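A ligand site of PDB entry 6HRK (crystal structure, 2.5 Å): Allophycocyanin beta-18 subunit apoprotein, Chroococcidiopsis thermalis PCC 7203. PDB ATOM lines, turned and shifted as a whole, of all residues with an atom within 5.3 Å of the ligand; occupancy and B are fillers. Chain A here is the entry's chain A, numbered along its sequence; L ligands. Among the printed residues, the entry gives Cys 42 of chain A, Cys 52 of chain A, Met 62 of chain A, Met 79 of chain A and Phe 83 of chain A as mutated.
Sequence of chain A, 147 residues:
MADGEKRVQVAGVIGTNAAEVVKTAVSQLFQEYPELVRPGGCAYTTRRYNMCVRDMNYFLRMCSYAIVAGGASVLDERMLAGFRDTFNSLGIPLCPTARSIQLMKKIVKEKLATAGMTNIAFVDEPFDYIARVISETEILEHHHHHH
The side-chain sulfur (SG) of Cys 42 is bonded to a carbon (C24) of the ligand, at 1.6 Å. A carbon (C23) of the ligand is covalently linked to the side-chain sulfur (SG) of Cys 52 (1.6 Å). The side-chain carboxylate (OD2) of Asp 55 sits at hydrogen-bond distance from a nitrogen (N3) of the ligand, 2.7 Å away. NH1 of Arg 54 is in salt-bridge range of O1 of the ligand (2.9 Å).
The guanidinium group (NH2) of Arg 54 is in salt-bridge range of the side-chain carboxylate (OD1) of Asp 55 (2.8 Å). The backbone carbonyl oxygen (O) of Phe 87 is in hydrogen-bond range of the backbone NH (N) of Ile 92, at 2.8 Å. The side-chain hydroxyl (OG) of Ser 100 sits at hydrogen-bond distance from the backbone carbonyl oxygen (O) of Thr 97 (2.6 Å). The backbone carbonyl oxygen (O) of Pro 96 is in hydrogen-bond range of the side-chain hydroxyl (OG) of Ser 100 (3.4 Å).
Merely in contact with the ligand: Arg 48, Met 51, Met 56, Tyr 58, Phe 59, Met 62, Phe 83, Phe 87, Leu 90, Ile 92, Thr 97 and Ser 100. Of the 22 residues printed, 16 come within 4 Å of the ligand. The nearest printed residue that does not touch the ligand is Leu 36 (4.2 Å).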
ATOM      1  N   LEU A  29      12.781  20.622  24.705  1.00  0.00           N
ATOM      2  CA  LEU A  29      13.933  20.420  25.591  1.00  0.00           C
ATOM      3  C   LEU A  29      13.506  19.907  26.978  1.00  0.00           C
ATOM      4  O   LEU A  29      14.121  18.972  27.497  1.00  0.00           O
ATOM      5  CB  LEU A  29      14.729  21.728  25.746  1.00  0.00           C
ATOM      6  CG  LEU A  29      16.056  21.685  26.530  1.00  0.00           C
ATOM      7  CD1 LEU A  29      17.118  20.913  25.757  1.00  0.00           C
ATOM      8  CD2 LEU A  29      16.532  23.088  26.846  1.00  0.00           C
ATOM      9  N   LEU A  36      15.497  20.114  34.197  1.00  0.00           N
ATOM     10  CA  LEU A  36      15.667  21.564  34.097  1.00  0.00           C
ATOM     11  C   LEU A  36      14.540  22.368  34.772  1.00  0.00           C
ATOM     12  O   LEU A  36      14.771  23.478  35.234  1.00  0.00           O
ATOM     13  CB  LEU A  36      15.811  22.010  32.639  1.00  0.00           C
ATOM     14  CG  LEU A  36      16.866  21.333  31.749  1.00  0.00           C
ATOM     15  CD1 LEU A  36      17.064  22.136  30.474  1.00  0.00           C
ATOM     16  CD2 LEU A  36      18.193  21.128  32.465  1.00  0.00           C
ATOM     17  N   CYS A  42      18.370  24.364  35.529  1.00  0.00           N
ATOM     18  CA  CYS A  42      18.631  25.731  35.059  1.00  0.00           C
ATOM     19  C   CYS A  42      17.392  26.462  34.493  1.00  0.00           C
ATOM     20  O   CYS A  42      17.538  27.457  33.767  1.00  0.00           O
ATOM     21  CB  CYS A  42      19.771  25.707  34.037  1.00  0.00           C
ATOM     22  SG  CYS A  42      19.518  24.586  32.643  1.00  0.00           S
ATOM     23  N   ALA A  43      16.190  25.977  34.799  1.00  0.00           N
ATOM     24  CA  ALA A  43      14.955  26.730  34.539  1.00  0.00           C
ATOM     25  C   ALA A  43      13.848  26.450  35.573  1.00  0.00           C
ATOM     26  O   ALA A  43      12.658  26.497  35.238  1.00  0.00           O
ATOM     27  CB  ALA A  43      14.460  26.430  33.128  1.00  0.00           C
ATOM     28  N   ARG A  48      15.400  31.977  36.468  1.00  0.00           N
ATOM     29  CA  ARG A  48      16.233  31.027  35.712  1.00  0.00           C
ATOM     30  C   ARG A  48      15.654  30.710  34.333  1.00  0.00           C
ATOM     31  O   ARG A  48      16.413  30.640  33.366  1.00  0.00           O
ATOM     32  CB  ARG A  48      16.432  29.724  36.502  1.00  0.00           C
ATOM     33  CG  ARG A  48      17.313  29.886  37.724  1.00  0.00           C
ATOM     34  CD  ARG A  48      17.317  28.628  38.562  1.00  0.00           C
ATOM     35  NE  ARG A  48      18.285  28.710  39.656  1.00  0.00           N
ATOM     36  CZ  ARG A  48      18.349  27.878  40.697  1.00  0.00           C
ATOM     37  NH1 ARG A  48      17.496  26.861  40.833  1.00  0.00           N
ATOM     38  NH2 ARG A  48      19.288  28.075  41.625  1.00  0.00           N
ATOM     39  N   MET A  51      16.256  33.684  31.941  1.00  0.00           N
ATOM     40  CA  MET A  51      17.652  33.652  31.509  1.00  0.00           C
ATOM     41  C   MET A  51      17.960  32.447  30.590  1.00  0.00           C
ATOM     42  O   MET A  51      18.868  32.523  29.759  1.00  0.00           O
ATOM     43  CB  MET A  51      18.612  33.676  32.710  1.00  0.00           C
ATOM     44  CG  MET A  51      18.610  35.010  33.436  1.00  0.00           C
ATOM     45  SD  MET A  51      19.794  35.105  34.793  1.00  0.00           S
ATOM     46  CE  MET A  51      19.033  33.976  35.952  1.00  0.00           C
ATOM     47  N   CYS A  52      17.207  31.360  30.749  1.00  0.00           N
ATOM     48  CA  CYS A  52      17.318  30.176  29.884  1.00  0.00           C
ATOM     49  C   CYS A  52      16.823  30.403  28.451  1.00  0.00           C
ATOM     50  O   CYS A  52      17.471  29.943  27.515  1.00  0.00           O
ATOM     51  CB  CYS A  52      16.612  28.971  30.531  1.00  0.00           C
ATOM     52  SG  CYS A  52      17.169  27.348  29.953  1.00  0.00           S
ATOM     53  N   ARG A  54      16.565  33.531  27.236  1.00  0.00           N
ATOM     54  CA  ARG A  54      17.516  34.582  26.873  1.00  0.00           C
ATOM     55  C   ARG A  54      18.791  33.983  26.257  1.00  0.00           C
ATOM     56  O   ARG A  54      19.219  34.399  25.181  1.00  0.00           O
ATOM     57  CB  ARG A  54      17.866  35.430  28.094  1.00  0.00           C
ATOM     58  CG  ARG A  54      18.804  36.613  27.869  1.00  0.00           C
ATOM     59  CD  ARG A  54      19.526  36.996  29.154  1.00  0.00           C
ATOM     60  NE  ARG A  54      20.540  36.011  29.527  1.00  0.00           N
ATOM     61  CZ  ARG A  54      21.464  36.174  30.476  1.00  0.00           C
ATOM     62  NH1 ARG A  54      21.537  37.285  31.198  1.00  0.00           N
ATOM     63  NH2 ARG A  54      22.324  35.190  30.701  1.00  0.00           N
ATOM     64  N   ASP A  55      19.379  33.015  26.962  1.00  0.00           N
ATOM     65  CA  ASP A  55      20.586  32.323  26.476  1.00  0.00           C
ATOM     66  C   ASP A  55      20.378  31.650  25.124  1.00  0.00           C
ATOM     67  O   ASP A  55      21.189  31.808  24.219  1.00  0.00           O
ATOM     68  CB  ASP A  55      21.062  31.268  27.485  1.00  0.00           C
ATOM     69  CG  ASP A  55      21.781  31.866  28.672  1.00  0.00           C
ATOM     70  OD1 ASP A  55      21.722  33.096  28.882  1.00  0.00           O
ATOM     71  OD2 ASP A  55      22.394  31.083  29.416  1.00  0.00           O
ATOM     72  N   MET A  56      19.286  30.894  24.993  1.00  0.00           N
ATOM     73  CA  MET A  56      18.939  30.252  23.719  1.00  0.00           C
ATOM     74  C   MET A  56      18.774  31.281  22.605  1.00  0.00           C
ATOM     75  O   MET A  56      19.198  31.041  21.471  1.00  0.00           O
ATOM     76  CB  MET A  56      17.668  29.427  23.862  1.00  0.00           C
ATOM     77  CG  MET A  56      17.885  28.148  24.652  1.00  0.00           C
ATOM     78  SD  MET A  56      16.353  27.248  24.926  1.00  0.00           S
ATOM     79  CE  MET A  56      15.994  26.696  23.256  1.00  0.00           C
ATOM     80  N   TYR A  58      20.337  34.200  22.538  1.00  0.00           N
ATOM     81  CA  TYR A  58      21.733  34.582  22.220  1.00  0.00           C
ATOM     82  C   TYR A  58      22.393  33.611  21.234  1.00  0.00           C
ATOM     83  O   TYR A  58      23.079  34.053  20.312  1.00  0.00           O
ATOM     84  CB  TYR A  58      22.622  34.637  23.475  1.00  0.00           C
ATOM     85  CG  TYR A  58      22.460  35.842  24.381  1.00  0.00           C
ATOM     86  CD1 TYR A  58      22.358  37.135  23.862  1.00  0.00           C
ATOM     87  CD2 TYR A  58      22.466  35.697  25.776  1.00  0.00           C
ATOM     88  CE1 TYR A  58      22.235  38.233  24.708  1.00  0.00           C
ATOM     89  CE2 TYR A  58      22.344  36.781  26.619  1.00  0.00           C
ATOM     90  CZ  TYR A  58      22.226  38.053  26.083  1.00  0.00           C
ATOM     91  OH  TYR A  58      22.112  39.139  26.922  1.00  0.00           O
ATOM     92  N   PHE A  59      22.194  32.306  21.426  1.00  0.00           N
ATOM     93  CA  PHE A  59      22.833  31.298  20.572  1.00  0.00           C
ATOM     94  C   PHE A  59      22.265  31.280  19.154  1.00  0.00           C
ATOM     95  O   PHE A  59      23.025  31.211  18.188  1.00  0.00           O
ATOM     96  CB  PHE A  59      22.777  29.905  21.206  1.00  0.00           C
ATOM     97  CG  PHE A  59      23.641  29.758  22.436  1.00  0.00           C
ATOM     98  CD1 PHE A  59      25.008  29.992  22.375  1.00  0.00           C
ATOM     99  CD2 PHE A  59      23.087  29.364  23.648  1.00  0.00           C
ATOM    100  CE1 PHE A  59      25.808  29.858  23.496  1.00  0.00           C
ATOM    101  CE2 PHE A  59      23.885  29.226  24.786  1.00  0.00           C
ATOM    102  CZ  PHE A  59      25.249  29.471  24.704  1.00  0.00           C
ATOM    103  N   MET A  62      23.565  34.453  17.371  1.00  0.00           N
ATOM    104  CA  MET A  62      24.918  34.197  16.872  1.00  0.00           C
ATOM    105  C   MET A  62      24.918  33.376  15.594  1.00  0.00           C
ATOM    106  O   MET A  62      25.713  33.642  14.687  1.00  0.00           O
ATOM    107  CB  MET A  62      25.746  33.461  17.932  1.00  0.00           C
ATOM    108  CG  MET A  62      26.302  34.344  19.034  1.00  0.00           C
ATOM    109  SD  MET A  62      27.015  33.333  20.354  1.00  0.00           S
ATOM    110  CE  MET A  62      28.184  34.492  21.081  1.00  0.00           C
ATOM    111  N   MET A  79      35.459  33.203  23.506  1.00  0.00           N
ATOM    112  CA  MET A  79      34.212  33.670  24.115  1.00  0.00           C
ATOM    113  C   MET A  79      33.242  32.522  24.363  1.00  0.00           C
ATOM    114  O   MET A  79      32.608  32.451  25.428  1.00  0.00           O
ATOM    115  CB  MET A  79      33.549  34.734  23.235  1.00  0.00           C
ATOM    116  CG  MET A  79      32.469  35.540  23.931  1.00  0.00           C
ATOM    117  SD  MET A  79      31.304  36.279  22.775  1.00  0.00           S
ATOM    118  CE  MET A  79      32.398  37.233  21.736  1.00  0.00           C
ATOM    119  N   PHE A  83      32.031  30.653  27.990  1.00  0.00           N
ATOM    120  CA  PHE A  83      30.689  30.249  28.456  1.00  0.00           C
ATOM    121  C   PHE A  83      30.674  28.793  28.950  1.00  0.00           C
ATOM    122  O   PHE A  83      29.957  28.475  29.888  1.00  0.00           O
ATOM    123  CB  PHE A  83      29.624  30.410  27.355  1.00  0.00           C
ATOM    124  CG  PHE A  83      29.557  31.803  26.753  1.00  0.00           C
ATOM    125  CD1 PHE A  83      29.643  32.944  27.554  1.00  0.00           C
ATOM    126  CD2 PHE A  83      29.389  31.964  25.391  1.00  0.00           C
ATOM    127  CE1 PHE A  83      29.577  34.211  27.003  1.00  0.00           C
ATOM    128  CE2 PHE A  83      29.324  33.235  24.823  1.00  0.00           C
ATOM    129  CZ  PHE A  83      29.408  34.353  25.630  1.00  0.00           C
ATOM    130  N   THR A  86      31.992  28.953  32.468  1.00  0.00           N
ATOM    131  CA  THR A  86      30.976  29.598  33.290  1.00  0.00           C
ATOM    132  C   THR A  86      29.821  28.645  33.605  1.00  0.00           C
ATOM    133  O   THR A  86      29.394  28.535  34.749  1.00  0.00           O
ATOM    134  CB  THR A  86      30.414  30.858  32.588  1.00  0.00           C
ATOM    135  OG1 THR A  86      31.495  31.713  32.206  1.00  0.00           O
ATOM    136  CG2 THR A  86      29.448  31.619  33.484  1.00  0.00           C
ATOM    137  N   PHE A  87      29.332  27.953  32.576  1.00  0.00           N
ATOM    138  CA  PHE A  87      28.206  27.018  32.702  1.00  0.00           C
ATOM    139  C   PHE A  87      28.525  25.849  33.634  1.00  0.00           C
ATOM    140  O   PHE A  87      27.685  25.444  34.445  1.00  0.00           O
ATOM    141  CB  PHE A  87      27.772  26.501  31.329  1.00  0.00           C
ATOM    142  CG  PHE A  87      26.880  27.456  30.557  1.00  0.00           C
ATOM    143  CD1 PHE A  87      27.003  28.846  30.660  1.00  0.00           C
ATOM    144  CD2 PHE A  87      25.917  26.947  29.683  1.00  0.00           C
ATOM    145  CE1 PHE A  87      26.185  29.687  29.930  1.00  0.00           C
ATOM    146  CE2 PHE A  87      25.101  27.794  28.959  1.00  0.00           C
ATOM    147  CZ  PHE A  87      25.225  29.167  29.077  1.00  0.00           C
ATOM    148  N   LEU A  90      28.591  27.455  37.198  1.00  0.00           N
ATOM    149  CA  LEU A  90      27.229  27.781  37.668  1.00  0.00           C
ATOM    150  C   LEU A  90      26.240  26.593  37.659  1.00  0.00           C
ATOM    151  O   LEU A  90      25.082  26.773  38.014  1.00  0.00           O
ATOM    152  CB  LEU A  90      26.656  28.947  36.846  1.00  0.00           C
ATOM    153  CG  LEU A  90      27.454  30.248  36.817  1.00  0.00           C
ATOM    154  CD1 LEU A  90      26.804  31.254  35.873  1.00  0.00           C
ATOM    155  CD2 LEU A  90      27.604  30.856  38.205  1.00  0.00           C
ATOM    156  N   ILE A  92      25.067  24.837  35.061  1.00  0.00           N
ATOM    157  CA  ILE A  92      24.251  24.701  33.860  1.00  0.00           C
ATOM    158  C   ILE A  92      24.855  23.536  33.085  1.00  0.00           C
ATOM    159  O   ILE A  92      26.006  23.633  32.649  1.00  0.00           O
ATOM    160  CB  ILE A  92      24.275  25.989  33.002  1.00  0.00           C
ATOM    161  CG1 ILE A  92      23.697  27.176  33.790  1.00  0.00           C
ATOM    162  CG2 ILE A  92      23.484  25.786  31.713  1.00  0.00           C
ATOM    163  CD1 ILE A  92      24.036  28.529  33.223  1.00  0.00           C
ATOM    164  N   PRO A  96      22.420  19.331  27.689  1.00  0.00           N
ATOM    165  CA  PRO A  96      21.141  19.997  27.396  1.00  0.00           C
ATOM    166  C   PRO A  96      21.284  21.327  26.661  1.00  0.00           C
ATOM    167  O   PRO A  96      20.470  21.621  25.790  1.00  0.00           O
ATOM    168  CB  PRO A  96      20.534  20.237  28.787  1.00  0.00           C
ATOM    169  CG  PRO A  96      21.172  19.221  29.663  1.00  0.00           C
ATOM    170  CD  PRO A  96      22.558  19.041  29.129  1.00  0.00           C
ATOM    171  N   THR A  97      22.299  22.116  27.023  1.00  0.00           N
ATOM    172  CA  THR A  97      22.630  23.364  26.316  1.00  0.00           C
ATOM    173  C   THR A  97      22.943  23.086  24.847  1.00  0.00           C
ATOM    174  O   THR A  97      22.514  23.834  23.956  1.00  0.00           O
ATOM    175  CB  THR A  97      23.845  24.074  26.955  1.00  0.00           C
ATOM    176  OG1 THR A  97      23.628  24.253  28.363  1.00  0.00           O
ATOM    177  CG2 THR A  97      24.103  25.438  26.312  1.00  0.00           C
ATOM    178  N   SER A 100      19.588  22.052  23.081  1.00  0.00           N
ATOM    179  CA  SER A 100      18.737  23.218  22.822  1.00  0.00           C
ATOM    180  C   SER A 100      19.118  23.946  21.528  1.00  0.00           C
ATOM    181  O   SER A 100      18.242  24.364  20.767  1.00  0.00           O
ATOM    182  CB  SER A 100      18.763  24.191  24.003  1.00  0.00           C
ATOM    183  OG  SER A 100      20.079  24.661  24.264  1.00  0.00           O
HETATM  184  C1  LIG L   1      23.693  32.727  33.324  1.00  0.00           C
HETATM  185  N1  LIG L   1      24.382  32.708  30.808  1.00  0.00           N
HETATM  186  C2  LIG L   1      24.509  33.085  32.100  1.00  0.00           C
HETATM  187  C3  LIG L   1      25.686  33.990  32.197  1.00  0.00           C
HETATM  188  C4  LIG L   1      26.208  34.110  30.914  1.00  0.00           C
HETATM  189  C5  LIG L   1      25.340  33.282  30.029  1.00  0.00           C
HETATM  190  C6  LIG L   1      27.415  34.917  30.526  1.00  0.00           C
HETATM  191  C7  LIG L   1      26.210  34.649  33.458  1.00  0.00           C
HETATM  192  C8  LIG L   1      26.015  36.161  33.467  1.00  0.00           C
HETATM  193  C9  LIG L   1      24.576  36.559  33.214  1.00  0.00           C
HETATM  194  O1  LIG L   1      24.261  36.894  32.059  1.00  0.00           O
HETATM  195  O2  LIG L   1      23.775  36.531  34.169  1.00  0.00           O
HETATM  196  C10 LIG L   1      25.486  33.046  28.533  1.00  0.00           C
HETATM  197  N2  LIG L   1      25.699  35.567  28.034  1.00  0.00           N
HETATM  198  C11 LIG L   1      25.701  34.261  27.651  1.00  0.00           C
HETATM  199  C12 LIG L   1      25.938  34.147  26.263  1.00  0.00           C
HETATM  200  C13 LIG L   1      26.100  35.427  25.726  1.00  0.00           C
HETATM  201  C14 LIG L   1      25.933  36.269  26.925  1.00  0.00           C
HETATM  202  C15 LIG L   1      25.997  32.859  25.491  1.00  0.00           C
HETATM  203  O3  LIG L   1      26.011  37.753  26.926  1.00  0.00           O
HETATM  204  C16 LIG L   1      26.374  35.780  24.271  1.00  0.00           C
HETATM  205  C17 LIG L   1      26.031  37.221  23.947  1.00  0.00           C
HETATM  206  N3  LIG L   1      21.706  28.497  29.860  1.00  0.00           N
HETATM  207  C18 LIG L   1      21.582  27.799  28.728  1.00  0.00           C
HETATM  208  C19 LIG L   1      20.497  26.780  28.910  1.00  0.00           C
HETATM  209  C20 LIG L   1      19.663  27.522  29.949  1.00  0.00           C
HETATM  210  C21 LIG L   1      20.714  28.182  30.854  1.00  0.00           C
HETATM  211  C22 LIG L   1      19.750  26.445  27.621  1.00  0.00           C
HETATM  212  O4  LIG L   1      22.184  27.994  27.679  1.00  0.00           O
HETATM  213  C23 LIG L   1      18.530  26.720  30.591  1.00  0.00           C
HETATM  214  C24 LIG L   1      19.008  25.671  31.566  1.00  0.00           C
HETATM  215  C25 LIG L   1      20.163  29.438  31.535  1.00  0.00           C
HETATM  216  N4  LIG L   1      22.037  31.084  32.137  1.00  0.00           N
HETATM  217  C26 LIG L   1      21.006  30.259  32.475  1.00  0.00           C
HETATM  218  C27 LIG L   1      20.770  30.372  33.945  1.00  0.00           C
HETATM  219  C28 LIG L   1      21.785  31.321  34.417  1.00  0.00           C
HETATM  220  C29 LIG L   1      22.555  31.734  33.218  1.00  0.00           C
HETATM  221  C30 LIG L   1      19.731  29.662  34.773  1.00  0.00           C
HETATM  222  C31 LIG L   1      22.009  31.795  35.836  1.00  0.00           C
HETATM  223  C32 LIG L   1      22.792  30.780  36.658  1.00  0.00           C
HETATM  224  C33 LIG L   1      22.878  31.310  38.066  1.00  0.00           C
HETATM  225  O5  LIG L   1      23.981  31.726  38.466  1.00  0.00           O
HETATM  226  O6  LIG L   1      21.847  31.307  38.773  1.00  0.00           O
